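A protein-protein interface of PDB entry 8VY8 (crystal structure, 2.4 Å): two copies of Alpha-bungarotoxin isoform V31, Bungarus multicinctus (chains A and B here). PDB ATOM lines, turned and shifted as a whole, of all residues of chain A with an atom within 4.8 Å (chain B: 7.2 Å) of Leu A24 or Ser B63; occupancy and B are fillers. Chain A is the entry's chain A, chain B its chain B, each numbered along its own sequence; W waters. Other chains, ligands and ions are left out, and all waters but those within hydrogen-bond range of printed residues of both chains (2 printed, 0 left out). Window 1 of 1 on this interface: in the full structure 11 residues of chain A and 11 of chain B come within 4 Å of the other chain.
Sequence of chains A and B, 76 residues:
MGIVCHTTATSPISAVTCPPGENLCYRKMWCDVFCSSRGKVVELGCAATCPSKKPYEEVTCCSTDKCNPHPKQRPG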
ATOM      1  N   ILE A   3     -21.587   0.180 -31.351  1.00  0.00           N
ATOM      2  CA  ILE A   3     -20.904   1.281 -32.017  1.00  0.00           C
ATOM      3  C   ILE A   3     -19.502   1.455 -31.447  1.00  0.00           C
ATOM      4  O   ILE A   3     -19.277   1.294 -30.242  1.00  0.00           O
ATOM      5  CB  ILE A   3     -21.720   2.580 -31.883  1.00  0.00           C
ATOM      6  CG1 ILE A   3     -21.116   3.684 -32.746  1.00  0.00           C
ATOM      7  CG2 ILE A   3     -21.780   3.022 -30.434  1.00  0.00           C
ATOM      8  CD1 ILE A   3     -21.972   4.937 -32.812  1.00  0.00           C
ATOM      9  N   CYS A   5     -16.352   4.120 -30.894  1.00  0.00           N
ATOM     10  CA  CYS A   5     -16.183   5.553 -30.730  1.00  0.00           C
ATOM     11  C   CYS A   5     -14.771   5.833 -30.245  1.00  0.00           C
ATOM     12  O   CYS A   5     -14.195   5.046 -29.490  1.00  0.00           O
ATOM     13  CB  CYS A   5     -17.162   6.133 -29.704  1.00  0.00           C
ATOM     14  SG  CYS A   5     -18.919   5.981 -30.078  1.00  0.00           S
ATOM     15  N   GLY A  21     -25.630  -0.549 -24.136  1.00  0.00           N
ATOM     16  CA  GLY A  21     -26.516   0.547 -23.807  1.00  0.00           C
ATOM     17  C   GLY A  21     -25.992   1.934 -24.115  1.00  0.00           C
ATOM     18  O   GLY A  21     -26.770   2.893 -24.056  1.00  0.00           O
ATOM     19  N   GLU A  22     -24.709   2.077 -24.424  1.00  0.00           N
ATOM     20  CA  GLU A  22     -24.111   3.350 -24.824  1.00  0.00           C
ATOM     21  C   GLU A  22     -23.818   3.264 -26.320  1.00  0.00           C
ATOM     22  O   GLU A  22     -22.816   2.669 -26.726  1.00  0.00           O
ATOM     23  CB  GLU A  22     -22.843   3.631 -24.026  1.00  0.00           C
ATOM     24  CG  GLU A  22     -23.076   3.854 -22.547  1.00  0.00           C
ATOM     25  CD  GLU A  22     -21.811   4.241 -21.817  1.00  0.00           C
ATOM     26  OE1 GLU A  22     -20.830   4.617 -22.490  1.00  0.00           O
ATOM     27  OE2 GLU A  22     -21.794   4.173 -20.572  1.00  0.00           O
ATOM     28  N   ASN A  23     -24.701   3.826 -27.146  1.00  0.00           N
ATOM     29  CA  ASN A  23     -24.621   3.627 -28.590  1.00  0.00           C
ATOM     30  C   ASN A  23     -24.478   4.930 -29.376  1.00  0.00           C
ATOM     31  O   ASN A  23     -24.868   5.001 -30.545  1.00  0.00           O
ATOM     32  CB  ASN A  23     -25.847   2.854 -29.074  1.00  0.00           C
ATOM     33  CG  ASN A  23     -26.042   1.543 -28.340  1.00  0.00           C
ATOM     34  OD1 ASN A  23     -25.283   0.590 -28.522  1.00  0.00           O
ATOM     35  ND2 ASN A  23     -27.059   1.496 -27.488  1.00  0.00           N
ATOM     36  N   LEU A  24     -23.918   5.967 -28.760  1.00  0.00           N
ATOM     37  CA  LEU A  24     -23.580   7.196 -29.466  1.00  0.00           C
ATOM     38  C   LEU A  24     -22.225   7.672 -28.969  1.00  0.00           C
ATOM     39  O   LEU A  24     -21.835   7.392 -27.833  1.00  0.00           O
ATOM     40  CB  LEU A  24     -24.644   8.278 -29.279  1.00  0.00           C
ATOM     41  CG  LEU A  24     -24.824   9.066 -27.987  1.00  0.00           C
ATOM     42  CD1 LEU A  24     -23.882  10.251 -27.944  1.00  0.00           C
ATOM     43  CD2 LEU A  24     -26.289   9.488 -27.918  1.00  0.00           C
ATOM     44  N   CYS A  25     -21.521   8.409 -29.819  1.00  0.00           N
ATOM     45  CA  CYS A  25     -20.263   9.033 -29.446  1.00  0.00           C
ATOM     46  C   CYS A  25     -20.486  10.491 -29.061  1.00  0.00           C
ATOM     47  O   CYS A  25     -21.440  11.131 -29.507  1.00  0.00           O
ATOM     48  CB  CYS A  25     -19.270   8.963 -30.605  1.00  0.00           C
ATOM     49  SG  CYS A  25     -19.231   7.386 -31.505  1.00  0.00           S
ATOM     50  N   TYR A  26     -19.594  11.011 -28.219  1.00  0.00           N
ATOM     51  CA  TYR A  26     -19.639  12.414 -27.830  1.00  0.00           C
ATOM     52  C   TYR A  26     -18.220  12.960 -27.763  1.00  0.00           C
ATOM     53  O   TYR A  26     -17.295  12.266 -27.332  1.00  0.00           O
ATOM     54  CB  TYR A  26     -20.376  12.609 -26.484  1.00  0.00           C
ATOM     55  CG  TYR A  26     -19.554  12.341 -25.238  1.00  0.00           C
ATOM     56  CD1 TYR A  26     -18.714  13.313 -24.711  1.00  0.00           C
ATOM     57  CD2 TYR A  26     -19.637  11.121 -24.578  1.00  0.00           C
ATOM     58  CE1 TYR A  26     -17.967  13.074 -23.577  1.00  0.00           C
ATOM     59  CE2 TYR A  26     -18.895  10.873 -23.440  1.00  0.00           C
ATOM     60  CZ  TYR A  26     -18.061  11.854 -22.943  1.00  0.00           C
ATOM     61  OH  TYR A  26     -17.312  11.615 -21.812  1.00  0.00           O
ATOM     62  N   GLY A  45     -15.646   9.977 -25.682  1.00  0.00           N
ATOM     63  CA  GLY A  45     -16.070   8.705 -25.132  1.00  0.00           C
ATOM     64  C   GLY A  45     -17.391   8.261 -25.714  1.00  0.00           C
ATOM     65  O   GLY A  45     -17.879   8.810 -26.705  1.00  0.00           O
ATOM     66  N   CYS A  46     -17.963   7.250 -25.072  1.00  0.00           N
ATOM     67  CA  CYS A  46     -19.268   6.710 -25.411  1.00  0.00           C
ATOM     68  C   CYS A  46     -20.309   7.278 -24.457  1.00  0.00           C
ATOM     69  O   CYS A  46     -19.983   7.817 -23.397  1.00  0.00           O
ATOM     70  CB  CYS A  46     -19.255   5.181 -25.336  1.00  0.00           C
ATOM     71  SG  CYS A  46     -17.977   4.421 -26.350  1.00  0.00           S
ATOM     72  N   ALA A  47     -21.575   7.152 -24.841  1.00  0.00           N
ATOM     73  CA  ALA A  47     -22.653   7.593 -23.967  1.00  0.00           C
ATOM     74  C   ALA A  47     -23.975   7.033 -24.462  1.00  0.00           C
ATOM     75  O   ALA A  47     -24.137   6.740 -25.650  1.00  0.00           O
ATOM     76  CB  ALA A  47     -22.728   9.123 -23.887  1.00  0.00           C
ATOM     77  N   ALA A  48     -24.914   6.880 -23.525  1.00  0.00           N
ATOM     78  CA  ALA A  48     -26.286   6.544 -23.885  1.00  0.00           C
ATOM     79  C   ALA A  48     -27.054   7.798 -24.285  1.00  0.00           C
ATOM     80  O   ALA A  48     -27.691   7.833 -25.343  1.00  0.00           O
ATOM     81  CB  ALA A  48     -26.974   5.832 -22.718  1.00  0.00           C
ATOM     82  N   THR A  49     -26.975   8.844 -23.468  1.00  0.00           N
ATOM     83  CA  THR A  49     -27.606  10.127 -23.737  1.00  0.00           C
ATOM     84  C   THR A  49     -26.551  11.197 -23.978  1.00  0.00           C
ATOM     85  O   THR A  49     -25.434  11.122 -23.455  1.00  0.00           O
ATOM     86  CB  THR A  49     -28.504  10.558 -22.576  1.00  0.00           C
ATOM     87  OG1 THR A  49     -27.777  10.436 -21.349  1.00  0.00           O
ATOM     88  CG2 THR A  49     -29.752   9.694 -22.510  1.00  0.00           C
ATOM     89  N   CYS A  50     -26.908  12.180 -24.800  1.00  0.00           N
ATOM     90  CA  CYS A  50     -26.013  13.299 -25.069  1.00  0.00           C
ATOM     91  C   CYS A  50     -25.736  14.063 -23.775  1.00  0.00           C
ATOM     92  O   CYS A  50     -26.681  14.421 -23.058  1.00  0.00           O
ATOM     93  CB  CYS A  50     -26.630  14.235 -26.107  1.00  0.00           C
ATOM     94  SG  CYS A  50     -25.438  15.253 -27.005  1.00  0.00           S
ATOM     95  N   CYS A  61     -22.591  15.201 -30.433  1.00  0.00           N
ATOM     96  CA  CYS A  61     -23.092  13.844 -30.297  1.00  0.00           C
ATOM     97  C   CYS A  61     -23.378  13.307 -31.687  1.00  0.00           C
ATOM     98  O   CYS A  61     -23.969  14.002 -32.518  1.00  0.00           O
ATOM     99  CB  CYS A  61     -24.346  13.806 -29.425  1.00  0.00           C
ATOM    100  SG  CYS A  61     -24.024  13.941 -27.651  1.00  0.00           S
ATOM    101  N   CYS A  62     -22.990  12.057 -31.922  1.00  0.00           N
ATOM    102  CA  CYS A  62     -23.166  11.428 -33.220  1.00  0.00           C
ATOM    103  C   CYS A  62     -23.229   9.921 -33.027  1.00  0.00           C
ATOM    104  O   CYS A  62     -22.865   9.393 -31.972  1.00  0.00           O
ATOM    105  CB  CYS A  62     -22.044  11.821 -34.189  1.00  0.00           C
ATOM    106  SG  CYS A  62     -20.361  11.574 -33.572  1.00  0.00           S
ATOM    107  N   SER A  63     -23.697   9.226 -34.067  1.00  0.00           N
ATOM    108  CA  SER A  63     -24.035   7.814 -33.950  1.00  0.00           C
ATOM    109  C   SER A  63     -23.499   6.983 -35.113  1.00  0.00           C
ATOM    110  O   SER A  63     -24.096   5.963 -35.474  1.00  0.00           O
ATOM    111  CB  SER A  63     -25.548   7.631 -33.832  1.00  0.00           C
ATOM    112  OG  SER A  63     -26.213   8.232 -34.929  1.00  0.00           O
ATOM    113  N   GLY B   2     -28.414   0.964 -36.550  1.00  0.00           N
ATOM    114  CA  GLY B   2     -29.780   0.389 -36.384  1.00  0.00           C
ATOM    115  C   GLY B   2     -30.403   0.738 -35.046  1.00  0.00           C
ATOM    116  O   GLY B   2     -29.768   0.603 -34.001  1.00  0.00           O
ATOM    117  N   ILE B   3     -31.657   1.183 -35.079  1.00  0.00           N
ATOM    118  CA  ILE B   3     -32.359   1.610 -33.875  1.00  0.00           C
ATOM    119  C   ILE B   3     -33.797   1.941 -34.249  1.00  0.00           C
ATOM    120  O   ILE B   3     -34.059   2.486 -35.327  1.00  0.00           O
ATOM    121  CB  ILE B   3     -31.646   2.807 -33.219  1.00  0.00           C
ATOM    122  CG1 ILE B   3     -32.381   3.232 -31.951  1.00  0.00           C
ATOM    123  CG2 ILE B   3     -31.548   3.966 -34.198  1.00  0.00           C
ATOM    124  CD1 ILE B   3     -31.591   4.186 -31.085  1.00  0.00           C
ATOM    125  N   VAL B   4     -34.735   1.604 -33.369  1.00  0.00           N
ATOM    126  CA  VAL B   4     -36.151   1.906 -33.555  1.00  0.00           C
ATOM    127  C   VAL B   4     -36.511   3.138 -32.740  1.00  0.00           C
ATOM    128  O   VAL B   4     -36.081   3.271 -31.587  1.00  0.00           O
ATOM    129  CB  VAL B   4     -37.031   0.722 -33.119  1.00  0.00           C
ATOM    130  CG1 VAL B   4     -38.497   1.089 -33.273  1.00  0.00           C
ATOM    131  CG2 VAL B   4     -36.708  -0.526 -33.900  1.00  0.00           C
ATOM    132  N   CYS B   5     -37.263   4.064 -33.333  1.00  0.00           N
ATOM    133  CA  CYS B   5     -37.630   5.227 -32.541  1.00  0.00           C
ATOM    134  C   CYS B   5     -38.946   5.860 -32.952  1.00  0.00           C
ATOM    135  O   CYS B   5     -39.340   5.849 -34.121  1.00  0.00           O
ATOM    136  CB  CYS B   5     -36.518   6.265 -32.525  1.00  0.00           C
ATOM    137  SG  CYS B   5     -35.823   6.171 -30.878  1.00  0.00           S
ATOM    138  N   ASN B  23     -28.652   6.751 -36.312  1.00  0.00           N
ATOM    139  CA  ASN B  23     -28.718   5.712 -35.287  1.00  0.00           C
ATOM    140  C   ASN B  23     -28.927   6.271 -33.883  1.00  0.00           C
ATOM    141  O   ASN B  23     -28.567   5.615 -32.899  1.00  0.00           O
ATOM    142  CB  ASN B  23     -27.448   4.858 -35.309  1.00  0.00           C
ATOM    143  CG  ASN B  23     -27.176   4.252 -36.663  1.00  0.00           C
ATOM    144  OD1 ASN B  23     -27.973   3.461 -37.174  1.00  0.00           O
ATOM    145  ND2 ASN B  23     -26.041   4.617 -37.257  1.00  0.00           N
ATOM    146  N   LEU B  24     -29.518   7.456 -33.764  1.00  0.00           N
ATOM    147  CA  LEU B  24     -29.903   8.011 -32.477  1.00  0.00           C
ATOM    148  C   LEU B  24     -31.271   8.654 -32.627  1.00  0.00           C
ATOM    149  O   LEU B  24     -31.680   9.045 -33.722  1.00  0.00           O
ATOM    150  CB  LEU B  24     -28.885   9.022 -31.948  1.00  0.00           C
ATOM    151  CG  LEU B  24     -28.718  10.406 -32.566  1.00  0.00           C
ATOM    152  CD1 LEU B  24     -29.841  11.333 -32.191  1.00  0.00           C
ATOM    153  CD2 LEU B  24     -27.382  10.959 -32.084  1.00  0.00           C
ATOM    154  N   CYS B  25     -31.993   8.720 -31.522  1.00  0.00           N
ATOM    155  CA  CYS B  25     -33.274   9.400 -31.460  1.00  0.00           C
ATOM    156  C   CYS B  25     -33.180  10.756 -30.789  1.00  0.00           C
ATOM    157  O   CYS B  25     -32.277  11.029 -29.996  1.00  0.00           O
ATOM    158  CB  CYS B  25     -34.261   8.535 -30.709  1.00  0.00           C
ATOM    159  SG  CYS B  25     -33.952   6.842 -31.055  1.00  0.00           S
ATOM    160  N   ALA B  48     -28.709  11.387 -37.225  1.00  0.00           N
ATOM    161  CA  ALA B  48     -27.307  11.029 -37.045  1.00  0.00           C
ATOM    162  C   ALA B  48     -26.676  11.848 -35.923  1.00  0.00           C
ATOM    163  O   ALA B  48     -26.030  11.291 -35.028  1.00  0.00           O
ATOM    164  CB  ALA B  48     -26.531  11.231 -38.347  1.00  0.00           C
ATOM    165  N   CYS B  50     -27.142  14.963 -32.838  1.00  0.00           N
ATOM    166  CA  CYS B  50     -28.085  15.643 -31.961  1.00  0.00           C
ATOM    167  C   CYS B  50     -28.342  17.059 -32.473  1.00  0.00           C
ATOM    168  O   CYS B  50     -27.386  17.796 -32.748  1.00  0.00           O
ATOM    169  CB  CYS B  50     -27.541  15.685 -30.535  1.00  0.00           C
ATOM    170  SG  CYS B  50     -28.810  15.764 -29.247  1.00  0.00           S
ATOM    171  N   CYS B  61     -31.253  13.652 -26.266  1.00  0.00           N
ATOM    172  CA  CYS B  61     -30.820  12.651 -27.233  1.00  0.00           C
ATOM    173  C   CYS B  61     -30.480  11.360 -26.513  1.00  0.00           C
ATOM    174  O   CYS B  61     -29.941  11.377 -25.402  1.00  0.00           O
ATOM    175  CB  CYS B  61     -29.601  13.138 -28.038  1.00  0.00           C
ATOM    176  SG  CYS B  61     -29.967  14.112 -29.510  1.00  0.00           S
ATOM    177  N   CYS B  62     -30.834  10.247 -27.146  1.00  0.00           N
ATOM    178  CA  CYS B  62     -30.616   8.931 -26.574  1.00  0.00           C
ATOM    179  C   CYS B  62     -30.481   7.930 -27.710  1.00  0.00           C
ATOM    180  O   CYS B  62     -30.827   8.210 -28.861  1.00  0.00           O
ATOM    181  CB  CYS B  62     -31.754   8.543 -25.633  1.00  0.00           C
ATOM    182  SG  CYS B  62     -33.388   8.730 -26.371  1.00  0.00           S
ATOM    183  N   SER B  63     -29.959   6.750 -27.366  1.00  0.00           N
ATOM    184  CA  SER B  63     -29.529   5.785 -28.370  1.00  0.00           C
ATOM    185  C   SER B  63     -29.972   4.362 -28.049  1.00  0.00           C
ATOM    186  O   SER B  63     -29.314   3.400 -28.460  1.00  0.00           O
ATOM    187  CB  SER B  63     -28.007   5.816 -28.524  1.00  0.00           C
ATOM    188  OG  SER B  63     -27.369   5.539 -27.286  1.00  0.00           O
ATOM    189  N   THR B  64     -31.086   4.204 -27.347  1.00  0.00           N
ATOM    190  CA  THR B  64     -31.700   2.906 -27.127  1.00  0.00           C
ATOM    191  C   THR B  64     -33.079   2.915 -27.766  1.00  0.00           C
ATOM    192  O   THR B  64     -33.681   3.975 -27.955  1.00  0.00           O
ATOM    193  CB  THR B  64     -31.806   2.581 -25.638  1.00  0.00           C
ATOM    194  OG1 THR B  64     -32.280   3.731 -24.929  1.00  0.00           O
ATOM    195  CG2 THR B  64     -30.448   2.174 -25.096  1.00  0.00           C
ATOM    196  N   ASP B  65     -33.570   1.727 -28.115  1.00  0.00           N
ATOM    197  CA  ASP B  65     -34.825   1.624 -28.846  1.00  0.00           C
ATOM    198  C   ASP B  65     -35.942   2.350 -28.106  1.00  0.00           C
ATOM    199  O   ASP B  65     -36.069   2.246 -26.883  1.00  0.00           O
ATOM    200  CB  ASP B  65     -35.201   0.152 -29.048  1.00  0.00           C
ATOM    201  CG  ASP B  65     -34.262  -0.568 -30.001  1.00  0.00           C
ATOM    202  OD1 ASP B  65     -33.576   0.115 -30.788  1.00  0.00           O
ATOM    203  OD2 ASP B  65     -34.216  -1.818 -29.972  1.00  0.00           O
ATOM    204  N   LYS B  66     -36.736   3.115 -28.860  1.00  0.00           N
ATOM    205  CA  LYS B  66     -37.940   3.764 -28.336  1.00  0.00           C
ATOM    206  C   LYS B  66     -37.628   4.590 -27.093  1.00  0.00           C
ATOM    207  O   LYS B  66     -38.443   4.698 -26.174  1.00  0.00           O
ATOM    208  CB  LYS B  66     -39.021   2.722 -28.041  1.00  0.00           C
ATOM    209  CG  LYS B  66     -39.270   1.754 -29.201  1.00  0.00           C
ATOM    210  CD  LYS B  66     -40.574   0.979 -29.042  1.00  0.00           C
ATOM    211  CE  LYS B  66     -40.417  -0.203 -28.101  1.00  0.00           C
ATOM    212  NZ  LYS B  66     -41.689  -0.968 -27.962  1.00  0.00           N
ATOM    213  N   CYS B  67     -36.440   5.185 -27.061  1.00  0.00           N
ATOM    214  CA  CYS B  67     -36.023   5.986 -25.921  1.00  0.00           C
ATOM    215  C   CYS B  67     -36.521   7.425 -25.968  1.00  0.00           C
ATOM    216  O   CYS B  67     -36.296   8.166 -25.006  1.00  0.00           O
ATOM    217  CB  CYS B  67     -34.502   5.985 -25.834  1.00  0.00           C
ATOM    218  SG  CYS B  67     -33.742   6.908 -27.180  1.00  0.00           S
HETATM  219  O   HOH W   1     -29.482  14.707 -24.977  1.00  0.00           O
HETATM  220  O   HOH W   2     -24.697  17.142 -31.505  1.00  0.00           O
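The backbone carbonyl oxygen (O) of Ser A63 lies within hydrogen-bond range of the side-chain amide nitrogen (ND2) of Asn B23. O of Ala B48 is in hydrogen-bond range of OG of Ser A63 (3.1 Å). The backbone NH (N) of Cys B50 is in hydrogen-bond range of the backbone carbonyl oxygen (O) of Cys A61 (3.3 Å). The backbone carbonyl oxygen (O) of Cys B61 is in hydrogen-bond range of the backbone NH (N) of Cys A50 (3.2 Å). ND2 of Asn A23 lies within hydrogen-bond range of O of Ser B63. The side-chain hydroxyl of Ser B63 sits at hydrogen-bond distance from the backbone carbonyl oxygen of Ala A48, 3.0 Å away.
The side-chain sulfur of Cys B62 is disulfide-bonded to the side-chain sulfur of Cys B67, 2.0 Å away. The backbone NH (N) of Ala A47 sits at hydrogen-bond distance from the backbone carbonyl oxygen (O) of Leu A24 (3.0 Å). The backbone NH (N) of Cys A25 lies within hydrogen-bond range of the backbone carbonyl oxygen (O) of Cys A62 (2.7 Å). The side-chain sulfur of Cys A50 is disulfide-bonded to the side-chain sulfur of Cys A61 (2.0 Å). The side-chain sulfur (SG) of Cys B5 is disulfide-bonded to the side-chain sulfur (SG) of Cys B25 (2.0 Å). The side-chain sulfur of Cys A5 is disulfide-bonded to the side-chain sulfur of Cys A25 (2.0 Å).
Among the printed residues, pairs that only touch across the chains: Gly A21 with Thr B64 (3.9 Å), Leu A24 with Ser B63 (3.8 Å), Ala A47 with Ser B63 (3.8 Å), Ala A48 with Cys B62 (3.4 Å), Thr A49 with Cys B61 (3.1 Å), Thr A49 with Cys B62 (3.9 Å), Cys A62 with Ala B48 (3.4 Å) and Ser A63 with Leu B24 (3.6 Å).
Of chain B, only Ser B63 (3.8 Å) comes within 4 Å of Leu A24. Of the printed residues of chain A, Ser B63 touches Asn A23 (3.1 Å), Leu A24 (3.8 Å), Ala A47 (3.8 Å) and Ala A48 (3.0 Å). Printed residues of chain B within 4 Å of Ala A48: Cys B62 (3.4 Å) and Ser B63 (3.0 Å). Of the printed residues of chain B, Ser A63 touches Asn B23 (3.0 Å), Leu B24 (3.6 Å) and Ala B48 (3.1 Å). Gly B2 touches none of the printed residues of chain A. The nearest residue of chain B that does not touch Leu A24 is Cys B62 (4.5 Å). The nearest residue of chain A that does not touch Ser B63 is Gly A21 (4.2 Å). The nearest printed residue of chain B that does not touch Asn A23 is Thr B64 (4.2 Å).
Of the 16 printed residues of chain B, 8 touch a printed residue of chain A. Among the printed residues, 14 pairs touch across the chains. Among the printed residues, no Asp or Glu carboxylate lies within 4 Å of a Lys or Arg side-chain nitrogen of the other chain.
Asn A23 touches Ser B63, and with the chains exchanged Ser A63 touches Asn B23. Leu A24 touches Ser B63, and with the chains exchanged Ser A63 touches Leu B24. Ala A48 touches Cys B62, and with the chains exchanged Cys A62 touches Ala B48. Ala A48 touches Ser B63, and with the chains exchanged Ser A63 touches Ala B48. 10 positions are printed for both chains. Of the 14 pairs that touch across the chains among the printed residues, 10 have their exchanged pair printed and touching as well.
Water W1 bridges N of Cys B61 and O of Cys A50. Water W2 bridges the backbone carbonyl oxygen (O) of Cys B50 (3.0 Å) and the backbone NH (N) of Cys A61 (3.1 Å).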
